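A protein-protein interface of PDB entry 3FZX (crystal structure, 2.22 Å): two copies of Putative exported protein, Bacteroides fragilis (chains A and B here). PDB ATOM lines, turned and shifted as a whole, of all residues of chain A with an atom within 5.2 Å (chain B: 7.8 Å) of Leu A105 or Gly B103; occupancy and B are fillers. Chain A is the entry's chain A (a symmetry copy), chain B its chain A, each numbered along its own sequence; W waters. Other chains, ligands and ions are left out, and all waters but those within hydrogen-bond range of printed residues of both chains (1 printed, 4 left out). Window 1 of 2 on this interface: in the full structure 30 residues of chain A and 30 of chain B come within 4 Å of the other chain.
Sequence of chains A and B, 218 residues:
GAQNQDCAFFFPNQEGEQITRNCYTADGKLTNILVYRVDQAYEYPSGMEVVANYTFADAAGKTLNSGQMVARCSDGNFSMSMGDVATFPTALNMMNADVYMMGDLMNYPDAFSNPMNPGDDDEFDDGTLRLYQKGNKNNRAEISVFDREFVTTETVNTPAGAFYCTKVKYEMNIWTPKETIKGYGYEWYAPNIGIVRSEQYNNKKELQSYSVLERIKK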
ATOM      1  N   VAL A  70       3.836   8.674   0.388  1.00  0.00           N
ATOM      2  CA  VAL A  70       5.163   9.247   0.292  1.00  0.00           C
ATOM      3  C   VAL A  70       6.040   8.550  -0.736  1.00  0.00           C
ATOM      4  O   VAL A  70       5.995   7.330  -0.878  1.00  0.00           O
ATOM      5  CB  VAL A  70       5.823   9.245   1.682  1.00  0.00           C
ATOM      6  CG1 VAL A  70       7.264   9.722   1.612  1.00  0.00           C
ATOM      7  CG2 VAL A  70       4.998  10.134   2.606  1.00  0.00           C
ATOM      8  N   ARG A  72      10.240   8.827  -1.948  1.00  0.00           N
ATOM      9  CA  ARG A  72      11.493   9.337  -1.444  1.00  0.00           C
ATOM     10  C   ARG A  72      12.767   8.743  -2.025  1.00  0.00           C
ATOM     11  O   ARG A  72      12.809   7.592  -2.438  1.00  0.00           O
ATOM     12  CB  ARG A  72      11.584   9.209   0.089  1.00  0.00           C
ATOM     13  CG  ARG A  72      11.687   7.804   0.615  1.00  0.00           C
ATOM     14  CD  ARG A  72      12.186   7.682   2.079  1.00  0.00           C
ATOM     15  NE  ARG A  72      11.421   8.464   3.045  1.00  0.00           N
ATOM     16  CZ  ARG A  72      11.388   8.243   4.362  1.00  0.00           C
ATOM     17  NH1 ARG A  72      12.000   7.197   4.911  1.00  0.00           N
ATOM     18  NH2 ARG A  72      10.685   9.056   5.145  1.00  0.00           N
ATOM     19  N   SER A  79      12.440   4.877  -2.911  1.00  0.00           N
ATOM     20  CA  SER A  79      11.392   3.971  -2.462  1.00  0.00           C
ATOM     21  C   SER A  79      10.082   4.715  -2.330  1.00  0.00           C
ATOM     22  O   SER A  79      10.063   5.956  -2.375  1.00  0.00           O
ATOM     23  CB  SER A  79      11.780   3.288  -1.143  1.00  0.00           C
ATOM     24  OG  SER A  79      11.947   4.202  -0.064  1.00  0.00           O
ATOM     25  N   MET A  80       8.977   3.977  -2.226  1.00  0.00           N
ATOM     26  CA  MET A  80       7.678   4.602  -2.039  1.00  0.00           C
ATOM     27  C   MET A  80       6.621   3.669  -1.475  1.00  0.00           C
ATOM     28  O   MET A  80       6.759   2.447  -1.495  1.00  0.00           O
ATOM     29  CB  MET A  80       7.158   5.253  -3.338  1.00  0.00           C
ATOM     30  CG  MET A  80       6.776   4.270  -4.434  1.00  0.00           C
ATOM     31  SD  MET A  80       6.093   5.255  -6.055  1.00  0.00           S
ATOM     32  CE  MET A  80       6.403   3.785  -7.330  1.00  0.00           C
ATOM     33  N   SER A  81       5.562   4.285  -0.966  1.00  0.00           N
ATOM     34  CA  SER A  81       4.364   3.584  -0.530  1.00  0.00           C
ATOM     35  C   SER A  81       3.803   2.715  -1.634  1.00  0.00           C
ATOM     36  O   SER A  81       3.931   3.027  -2.826  1.00  0.00           O
ATOM     37  CB  SER A  81       3.277   4.591  -0.154  1.00  0.00           C
ATOM     38  OG  SER A  81       3.737   5.425   0.868  1.00  0.00           O
ATOM     39  N   GLY A 103       1.563  -0.337   4.393  1.00  0.00           N
ATOM     40  CA  GLY A 103       2.500  -1.187   3.709  1.00  0.00           C
ATOM     41  C   GLY A 103       3.913  -0.726   3.943  1.00  0.00           C
ATOM     42  O   GLY A 103       4.145   0.312   4.525  1.00  0.00           O
ATOM     43  N   ASP A 104       4.861  -1.518   3.475  1.00  0.00           N
ATOM     44  CA  ASP A 104       6.257  -1.118   3.439  1.00  0.00           C
ATOM     45  C   ASP A 104       6.453  -0.007   2.428  1.00  0.00           C
ATOM     46  O   ASP A 104       5.623   0.178   1.521  1.00  0.00           O
ATOM     47  CB  ASP A 104       7.108  -2.295   2.965  1.00  0.00           C
ATOM     48  CG  ASP A 104       6.996  -3.483   3.885  1.00  0.00           C
ATOM     49  OD1 ASP A 104       7.702  -3.445   4.928  1.00  0.00           O
ATOM     50  OD2 ASP A 104       6.172  -4.398   3.578  1.00  0.00           O
ATOM     51  N   LEU A 105       7.543   0.742   2.593  1.00  0.00           N
ATOM     52  CA  LEU A 105       8.016   1.596   1.520  1.00  0.00           C
ATOM     53  C   LEU A 105       8.772   0.581   0.659  1.00  0.00           C
ATOM     54  O   LEU A 105       9.632  -0.127   1.155  1.00  0.00           O
ATOM     55  CB  LEU A 105       8.949   2.701   2.026  1.00  0.00           C
ATOM     56  CG  LEU A 105       8.361   3.754   2.947  1.00  0.00           C
ATOM     57  CD1 LEU A 105       9.451   4.705   3.398  1.00  0.00           C
ATOM     58  CD2 LEU A 105       7.232   4.487   2.232  1.00  0.00           C
ATOM     59  N   MET A 106       8.417   0.484  -0.612  1.00  0.00           N
ATOM     60  CA  MET A 106       9.049  -0.443  -1.522  1.00  0.00           C
ATOM     61  C   MET A 106      10.030   0.280  -2.467  1.00  0.00           C
ATOM     62  O   MET A 106       9.714   1.336  -3.023  1.00  0.00           O
ATOM     63  CB  MET A 106       7.963  -1.134  -2.343  1.00  0.00           C
ATOM     64  CG  MET A 106       8.480  -2.243  -3.206  1.00  0.00           C
ATOM     65  SD  MET A 106       6.992  -3.477  -3.597  1.00  0.00           S
ATOM     66  CE  MET A 106       6.183  -2.453  -4.894  1.00  0.00           C
ATOM     67  N   ASN A 107      11.173  -0.344  -2.694  1.00  0.00           N
ATOM     68  CA  ASN A 107      12.255   0.243  -3.483  1.00  0.00           C
ATOM     69  C   ASN A 107      12.089   0.033  -4.998  1.00  0.00           C
ATOM     70  O   ASN A 107      11.508  -0.962  -5.430  1.00  0.00           O
ATOM     71  CB  ASN A 107      13.600  -0.316  -3.018  1.00  0.00           C
ATOM     72  CG  ASN A 107      13.806  -1.758  -3.468  1.00  0.00           C
ATOM     73  OD1 ASN A 107      12.950  -2.634  -3.251  1.00  0.00           O
ATOM     74  ND2 ASN A 107      14.898  -1.997  -4.153  1.00  0.00           N
ATOM     75  N   ARG B  72       3.417  -4.961  13.207  1.00  0.00           N
ATOM     76  CA  ARG B  72       2.989  -6.129  12.475  1.00  0.00           C
ATOM     77  C   ARG B  72       3.942  -7.314  12.441  1.00  0.00           C
ATOM     78  O   ARG B  72       5.154  -7.165  12.507  1.00  0.00           O
ATOM     79  CB  ARG B  72       2.629  -5.787  11.017  1.00  0.00           C
ATOM     80  CG  ARG B  72       3.786  -5.388  10.142  1.00  0.00           C
ATOM     81  CD  ARG B  72       3.510  -5.444   8.616  1.00  0.00           C
ATOM     82  NE  ARG B  72       2.342  -4.684   8.184  1.00  0.00           N
ATOM     83  CZ  ARG B  72       2.119  -4.257   6.938  1.00  0.00           C
ATOM     84  NH1 ARG B  72       3.018  -4.418   5.972  1.00  0.00           N
ATOM     85  NH2 ARG B  72       0.991  -3.609   6.661  1.00  0.00           N
ATOM     86  N   MET B  80       7.815  -2.614  12.618  1.00  0.00           N
ATOM     87  CA  MET B  80       6.955  -1.516  13.028  1.00  0.00           C
ATOM     88  C   MET B  80       7.466  -0.147  12.615  1.00  0.00           C
ATOM     89  O   MET B  80       8.634   0.032  12.274  1.00  0.00           O
ATOM     90  CB  MET B  80       6.681  -1.532  14.546  1.00  0.00           C
ATOM     91  CG  MET B  80       7.886  -1.207  15.415  1.00  0.00           C
ATOM     92  SD  MET B  80       7.377  -1.240  17.365  1.00  0.00           S
ATOM     93  CE  MET B  80       9.209  -1.480  18.049  1.00  0.00           C
ATOM     94  N   SER B  81       6.552   0.813  12.651  1.00  0.00           N
ATOM     95  CA  SER B  81       6.864   2.222  12.460  1.00  0.00           C
ATOM     96  C   SER B  81       7.937   2.682  13.422  1.00  0.00           C
ATOM     97  O   SER B  81       8.051   2.176  14.547  1.00  0.00           O
ATOM     98  CB  SER B  81       5.623   3.073  12.727  1.00  0.00           C
ATOM     99  OG  SER B  81       4.593   2.694  11.862  1.00  0.00           O
ATOM    100  N   MET B  82       8.688   3.687  12.990  1.00  0.00           N
ATOM    101  CA  MET B  82       9.859   4.161  13.716  1.00  0.00           C
ATOM    102  C   MET B  82       9.549   5.280  14.722  1.00  0.00           C
ATOM    103  O   MET B  82      10.453   5.983  15.161  1.00  0.00           O
ATOM    104  CB  MET B  82      10.909   4.625  12.695  1.00  0.00           C
ATOM    105  CG  MET B  82      11.513   3.506  11.879  1.00  0.00           C
ATOM    106  SD  MET B  82      12.666   4.290  10.516  1.00  0.00           S
ATOM    107  CE  MET B  82      14.128   4.939  11.711  1.00  0.00           C
ATOM    108  N   GLY B  83       8.277   5.459  15.071  1.00  0.00           N
ATOM    109  CA  GLY B  83       7.857   6.403  16.112  1.00  0.00           C
ATOM    110  C   GLY B  83       8.856   6.584  17.254  1.00  0.00           C
ATOM    111  O   GLY B  83       9.213   7.718  17.601  1.00  0.00           O
ATOM    112  N   MET B 101       5.306  12.878   9.992  1.00  0.00           N
ATOM    113  CA  MET B 101       6.486  12.054   9.900  1.00  0.00           C
ATOM    114  C   MET B 101       6.216  10.808   9.065  1.00  0.00           C
ATOM    115  O   MET B 101       5.082  10.353   8.968  1.00  0.00           O
ATOM    116  CB  MET B 101       7.001  11.723  11.287  1.00  0.00           C
ATOM    117  CG  MET B 101       5.995  11.110  12.179  1.00  0.00           C
ATOM    118  SD  MET B 101       6.703  10.942  13.983  1.00  0.00           S
ATOM    119  CE  MET B 101       6.021  12.604  14.795  1.00  0.00           C
ATOM    120  N   MET B 102       7.263  10.340   8.393  1.00  0.00           N
ATOM    121  CA  MET B 102       7.201   9.143   7.566  1.00  0.00           C
ATOM    122  C   MET B 102       8.532   8.415   7.731  1.00  0.00           C
ATOM    123  O   MET B 102       9.592   9.039   7.724  1.00  0.00           O
ATOM    124  CB  MET B 102       7.002   9.496   6.093  1.00  0.00           C
ATOM    125  CG  MET B 102       5.743  10.304   5.750  1.00  0.00           C
ATOM    126  SD  MET B 102       4.121   9.263   5.390  1.00  0.00           S
ATOM    127  CE  MET B 102       3.720   8.537   7.174  1.00  0.00           C
ATOM    128  N   GLY B 103       8.464   7.102   7.868  1.00  0.00           N
ATOM    129  CA  GLY B 103       9.633   6.271   7.971  1.00  0.00           C
ATOM    130  C   GLY B 103       9.363   4.896   7.421  1.00  0.00           C
ATOM    131  O   GLY B 103       8.246   4.564   7.083  1.00  0.00           O
ATOM    132  N   ASP B 104      10.410   4.095   7.337  1.00  0.00           N
ATOM    133  CA  ASP B 104      10.282   2.683   7.023  1.00  0.00           C
ATOM    134  C   ASP B 104       9.606   1.956   8.167  1.00  0.00           C
ATOM    135  O   ASP B 104       9.587   2.448   9.308  1.00  0.00           O
ATOM    136  CB  ASP B 104      11.674   2.069   6.878  1.00  0.00           C
ATOM    137  CG  ASP B 104      12.466   2.714   5.770  1.00  0.00           C
ATOM    138  OD1 ASP B 104      12.212   2.315   4.602  1.00  0.00           O
ATOM    139  OD2 ASP B 104      13.279   3.637   6.080  1.00  0.00           O
ATOM    140  N   LEU B 105       9.036   0.791   7.859  1.00  0.00           N
ATOM    141  CA  LEU B 105       8.665  -0.146   8.903  1.00  0.00           C
ATOM    142  C   LEU B 105      10.015  -0.812   9.183  1.00  0.00           C
ATOM    143  O   LEU B 105      10.658  -1.304   8.272  1.00  0.00           O
ATOM    144  CB  LEU B 105       7.629  -1.167   8.426  1.00  0.00           C
ATOM    145  CG  LEU B 105       6.252  -0.652   8.048  1.00  0.00           C
ATOM    146  CD1 LEU B 105       5.402  -1.795   7.531  1.00  0.00           C
ATOM    147  CD2 LEU B 105       5.611   0.029   9.252  1.00  0.00           C
ATOM    148  N   MET B 106      10.455  -0.783  10.430  1.00  0.00           N
ATOM    149  CA  MET B 106      11.719  -1.369  10.816  1.00  0.00           C
ATOM    150  C   MET B 106      11.513  -2.711  11.547  1.00  0.00           C
ATOM    151  O   MET B 106      10.655  -2.830  12.427  1.00  0.00           O
ATOM    152  CB  MET B 106      12.446  -0.391  11.736  1.00  0.00           C
ATOM    153  CG  MET B 106      13.843  -0.811  12.071  1.00  0.00           C
ATOM    154  SD  MET B 106      14.871   0.790  12.588  1.00  0.00           S
ATOM    155  CE  MET B 106      14.200   0.948  14.295  1.00  0.00           C
ATOM    156  N   GLY B 127      16.941   2.146   8.784  1.00  0.00           N
ATOM    157  CA  GLY B 127      15.721   2.878   8.496  1.00  0.00           C
ATOM    158  C   GLY B 127      15.919   4.356   8.640  1.00  0.00           C
ATOM    159  O   GLY B 127      16.808   4.781   9.377  1.00  0.00           O
ATOM    160  N   THR B 128      15.089   5.124   7.923  1.00  0.00           N
ATOM    161  CA  THR B 128      15.152   6.582   7.947  1.00  0.00           C
ATOM    162  C   THR B 128      13.771   7.171   8.246  1.00  0.00           C
ATOM    163  O   THR B 128      12.775   6.820   7.612  1.00  0.00           O
ATOM    164  CB  THR B 128      15.695   7.124   6.630  1.00  0.00           C
ATOM    165  OG1 THR B 128      16.987   6.560   6.429  1.00  0.00           O
ATOM    166  CG2 THR B 128      15.794   8.651   6.642  1.00  0.00           C
ATOM    167  N   LEU B 129      13.729   8.023   9.259  1.00  0.00           N
ATOM    168  CA  LEU B 129      12.536   8.755   9.633  1.00  0.00           C
ATOM    169  C   LEU B 129      12.750  10.211   9.258  1.00  0.00           C
ATOM    170  O   LEU B 129      13.779  10.791   9.599  1.00  0.00           O
ATOM    171  CB  LEU B 129      12.294   8.635  11.147  1.00  0.00           C
ATOM    172  CG  LEU B 129      11.074   9.343  11.717  1.00  0.00           C
ATOM    173  CD1 LEU B 129       9.755   8.738  11.230  1.00  0.00           C
ATOM    174  CD2 LEU B 129      11.195   9.334  13.232  1.00  0.00           C
ATOM    175  N   ARG B 130      11.774  10.796   8.564  1.00  0.00           N
ATOM    176  CA  ARG B 130      11.792  12.218   8.228  1.00  0.00           C
ATOM    177  C   ARG B 130      10.580  12.899   8.859  1.00  0.00           C
ATOM    178  O   ARG B 130       9.471  12.367   8.796  1.00  0.00           O
ATOM    179  CB  ARG B 130      11.811  12.404   6.706  1.00  0.00           C
ATOM    180  CG  ARG B 130      13.201  12.016   6.096  1.00  0.00           C
ATOM    181  CD  ARG B 130      13.150  11.923   4.625  1.00  0.00           C
ATOM    182  NE  ARG B 130      14.476  11.804   4.022  1.00  0.00           N
ATOM    183  CZ  ARG B 130      14.722  11.672   2.724  1.00  0.00           C
ATOM    184  NH1 ARG B 130      13.729  11.594   1.842  1.00  0.00           N
ATOM    185  NH2 ARG B 130      15.978  11.609   2.298  1.00  0.00           N
ATOM    186  N   LEU B 131      10.805  14.062   9.481  1.00  0.00           N
ATOM    187  CA  LEU B 131       9.734  14.857  10.070  1.00  0.00           C
ATOM    188  C   LEU B 131       9.701  16.213   9.375  1.00  0.00           C
ATOM    189  O   LEU B 131      10.727  16.739   8.949  1.00  0.00           O
ATOM    190  CB  LEU B 131       9.927  15.027  11.583  1.00  0.00           C
ATOM    191  CG  LEU B 131      10.112  13.724  12.369  1.00  0.00           C
ATOM    192  CD1 LEU B 131      11.565  13.307  12.437  1.00  0.00           C
ATOM    193  CD2 LEU B 131       9.537  13.847  13.768  1.00  0.00           C
ATOM    194  N   TYR B 132       8.515  16.765   9.216  1.00  0.00           N
ATOM    195  CA  TYR B 132       8.378  18.067   8.553  1.00  0.00           C
ATOM    196  C   TYR B 132       7.096  18.723   8.966  1.00  0.00           C
ATOM    197  O   TYR B 132       6.103  18.051   9.159  1.00  0.00           O
ATOM    198  CB  TYR B 132       8.375  17.942   7.027  1.00  0.00           C
ATOM    199  CG  TYR B 132       7.984  16.587   6.518  1.00  0.00           C
ATOM    200  CD1 TYR B 132       6.648  16.230   6.286  1.00  0.00           C
ATOM    201  CD2 TYR B 132       8.984  15.650   6.260  1.00  0.00           C
ATOM    202  CE1 TYR B 132       6.346  14.947   5.826  1.00  0.00           C
ATOM    203  CE2 TYR B 132       8.704  14.392   5.811  1.00  0.00           C
ATOM    204  CZ  TYR B 132       7.410  14.032   5.597  1.00  0.00           C
ATOM    205  OH  TYR B 132       7.277  12.753   5.148  1.00  0.00           O
ATOM    206  N   ILE B 143      16.138  11.521  10.643  1.00  0.00           N
ATOM    207  CA  ILE B 143      16.866  10.636  11.580  1.00  0.00           C
ATOM    208  C   ILE B 143      17.154   9.297  10.897  1.00  0.00           C
ATOM    209  O   ILE B 143      16.232   8.523  10.601  1.00  0.00           O
ATOM    210  CB  ILE B 143      16.115  10.366  12.899  1.00  0.00           C
ATOM    211  CG1 ILE B 143      15.740  11.676  13.620  1.00  0.00           C
ATOM    212  CG2 ILE B 143      17.024   9.536  13.863  1.00  0.00           C
ATOM    213  CD1 ILE B 143      14.715  11.495  14.748  1.00  0.00           C
HETATM  214  O   HOH W   1      12.809   2.810   2.027  1.00  0.00           O
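Arg A72 touches Gly B103, and with the chains exchanged Gly A103 touches Arg B72. Arg A72 touches Asp B104, and with the chains exchanged Asp A104 touches Arg B72. Gly A103 touches Leu B105, and with the chains exchanged Leu A105 touches Gly B103. Asp A104 touches Leu B105, and with the chains exchanged Leu A105 touches Asp B104. Of the 12 pairs that touch across the chains among the printed residues, 8 have their exchanged pair printed and touching as well.
The backbone carbonyl oxygen (O) of Val A70 lies within hydrogen-bond range of the backbone NH (N) of Ser A81, at 3.1 Å. The backbone NH (N) of Thr B128 is in hydrogen-bond range of the side-chain carboxylate (OD2) of Asp B104. O of Met B102 sits at hydrogen-bond distance from N of Arg B130, at 2.9 Å. N of Thr B128 is in hydrogen-bond range of SD of Met B82 (3.6 Å). The backbone carbonyl oxygen of Arg A72 lies within hydrogen-bond range of the backbone NH of Ser A79, at 2.8 Å.
The guanidinium group (NH1) of Arg B72 lies within salt-bridge range of the side-chain carboxylate (OD2) of Asp A104. The guanidinium group (NH1) of Arg A72 is in salt-bridge range of the side-chain carboxylate (OD2) of Asp B104 (3.96 Å). The backbone carbonyl oxygen (O) of Thr B128 sits at hydrogen-bond distance from the guanidinium group (NH1) of Arg A72. O of Met B102 is in hydrogen-bond range of NH2 of Arg A72 (2.8 Å).
Water W1 bridges the side-chain hydroxyl of Ser A79 (2.7 Å) and the side-chain carboxylate of Asp B104 (2.7 Å).
Of the printed residues of chain B, Val A70 touches Met B102. Of the printed residues of chain B, Arg A72 touches Met B102 (2.8 Å), Gly B103 (3.98 Å), Asp B104 (3.96 Å), Thr B128 (2.8 Å) and Arg B130 (3.7 Å). Ser A81 touches none of the printed residues of chain B. Of the printed residues of chain B, Gly A103 touches Arg B72 and Leu B105. Printed residues of chain B within 4 Å of Leu A105: Gly B103 (3.9 Å) and Asp B104 (3.8 Å). Met B82 touches none of the printed residues of chain A. Of the printed residues of chain A, Met B102 touches Val A70 (3.0 Å) and Arg A72 (2.8 Å). Gly B103 touches just these residues of chain A: Arg A72 and Leu A105. Printed residues of chain A within 4 Å of Thr B128: Arg A72 (2.8 Å). The nearest printed residue of chain A that does not touch Gly B103 is Gly A103 (6.4 Å). The nearest printed residue of chain B that does not touch Arg A72 is Leu B129 (4.7 Å).
Of the 10 printed residues of chain A, 5 touch a printed residue of chain B. Printed residues of chain A that touch a printed residue of chain B: Val A70, Arg A72, Gly A103, Asp A104 and Leu A105. Hydrophobic or aromatic side chains of chain A within 4 Å of the printed part of chain B: Val A70 and Leu A105. Among the printed residues, Asp or Glu carboxylates within 4 Å of a Lys or Arg side-chain nitrogen of the other chain: Arg A72 with Asp B104 and Asp A104 with Arg B72.
CG2 of Val A70 touches SD of Met B102 (3.0 Å). NH1 of Arg A72 touches CA of Gly B103, 3.98 Å away. Arg B130 touches Arg A72. Gly A103 touches Arg B72. Leu B105 touches Gly A103 (CD1 to O, 3.9 Å). Leu B105 touches Asp A104. CD1 of Leu A105 touches O of Gly B103 (3.9 Å). Leu A105 touches Asp B104 (CD1 to OD1, 3.8 Å).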
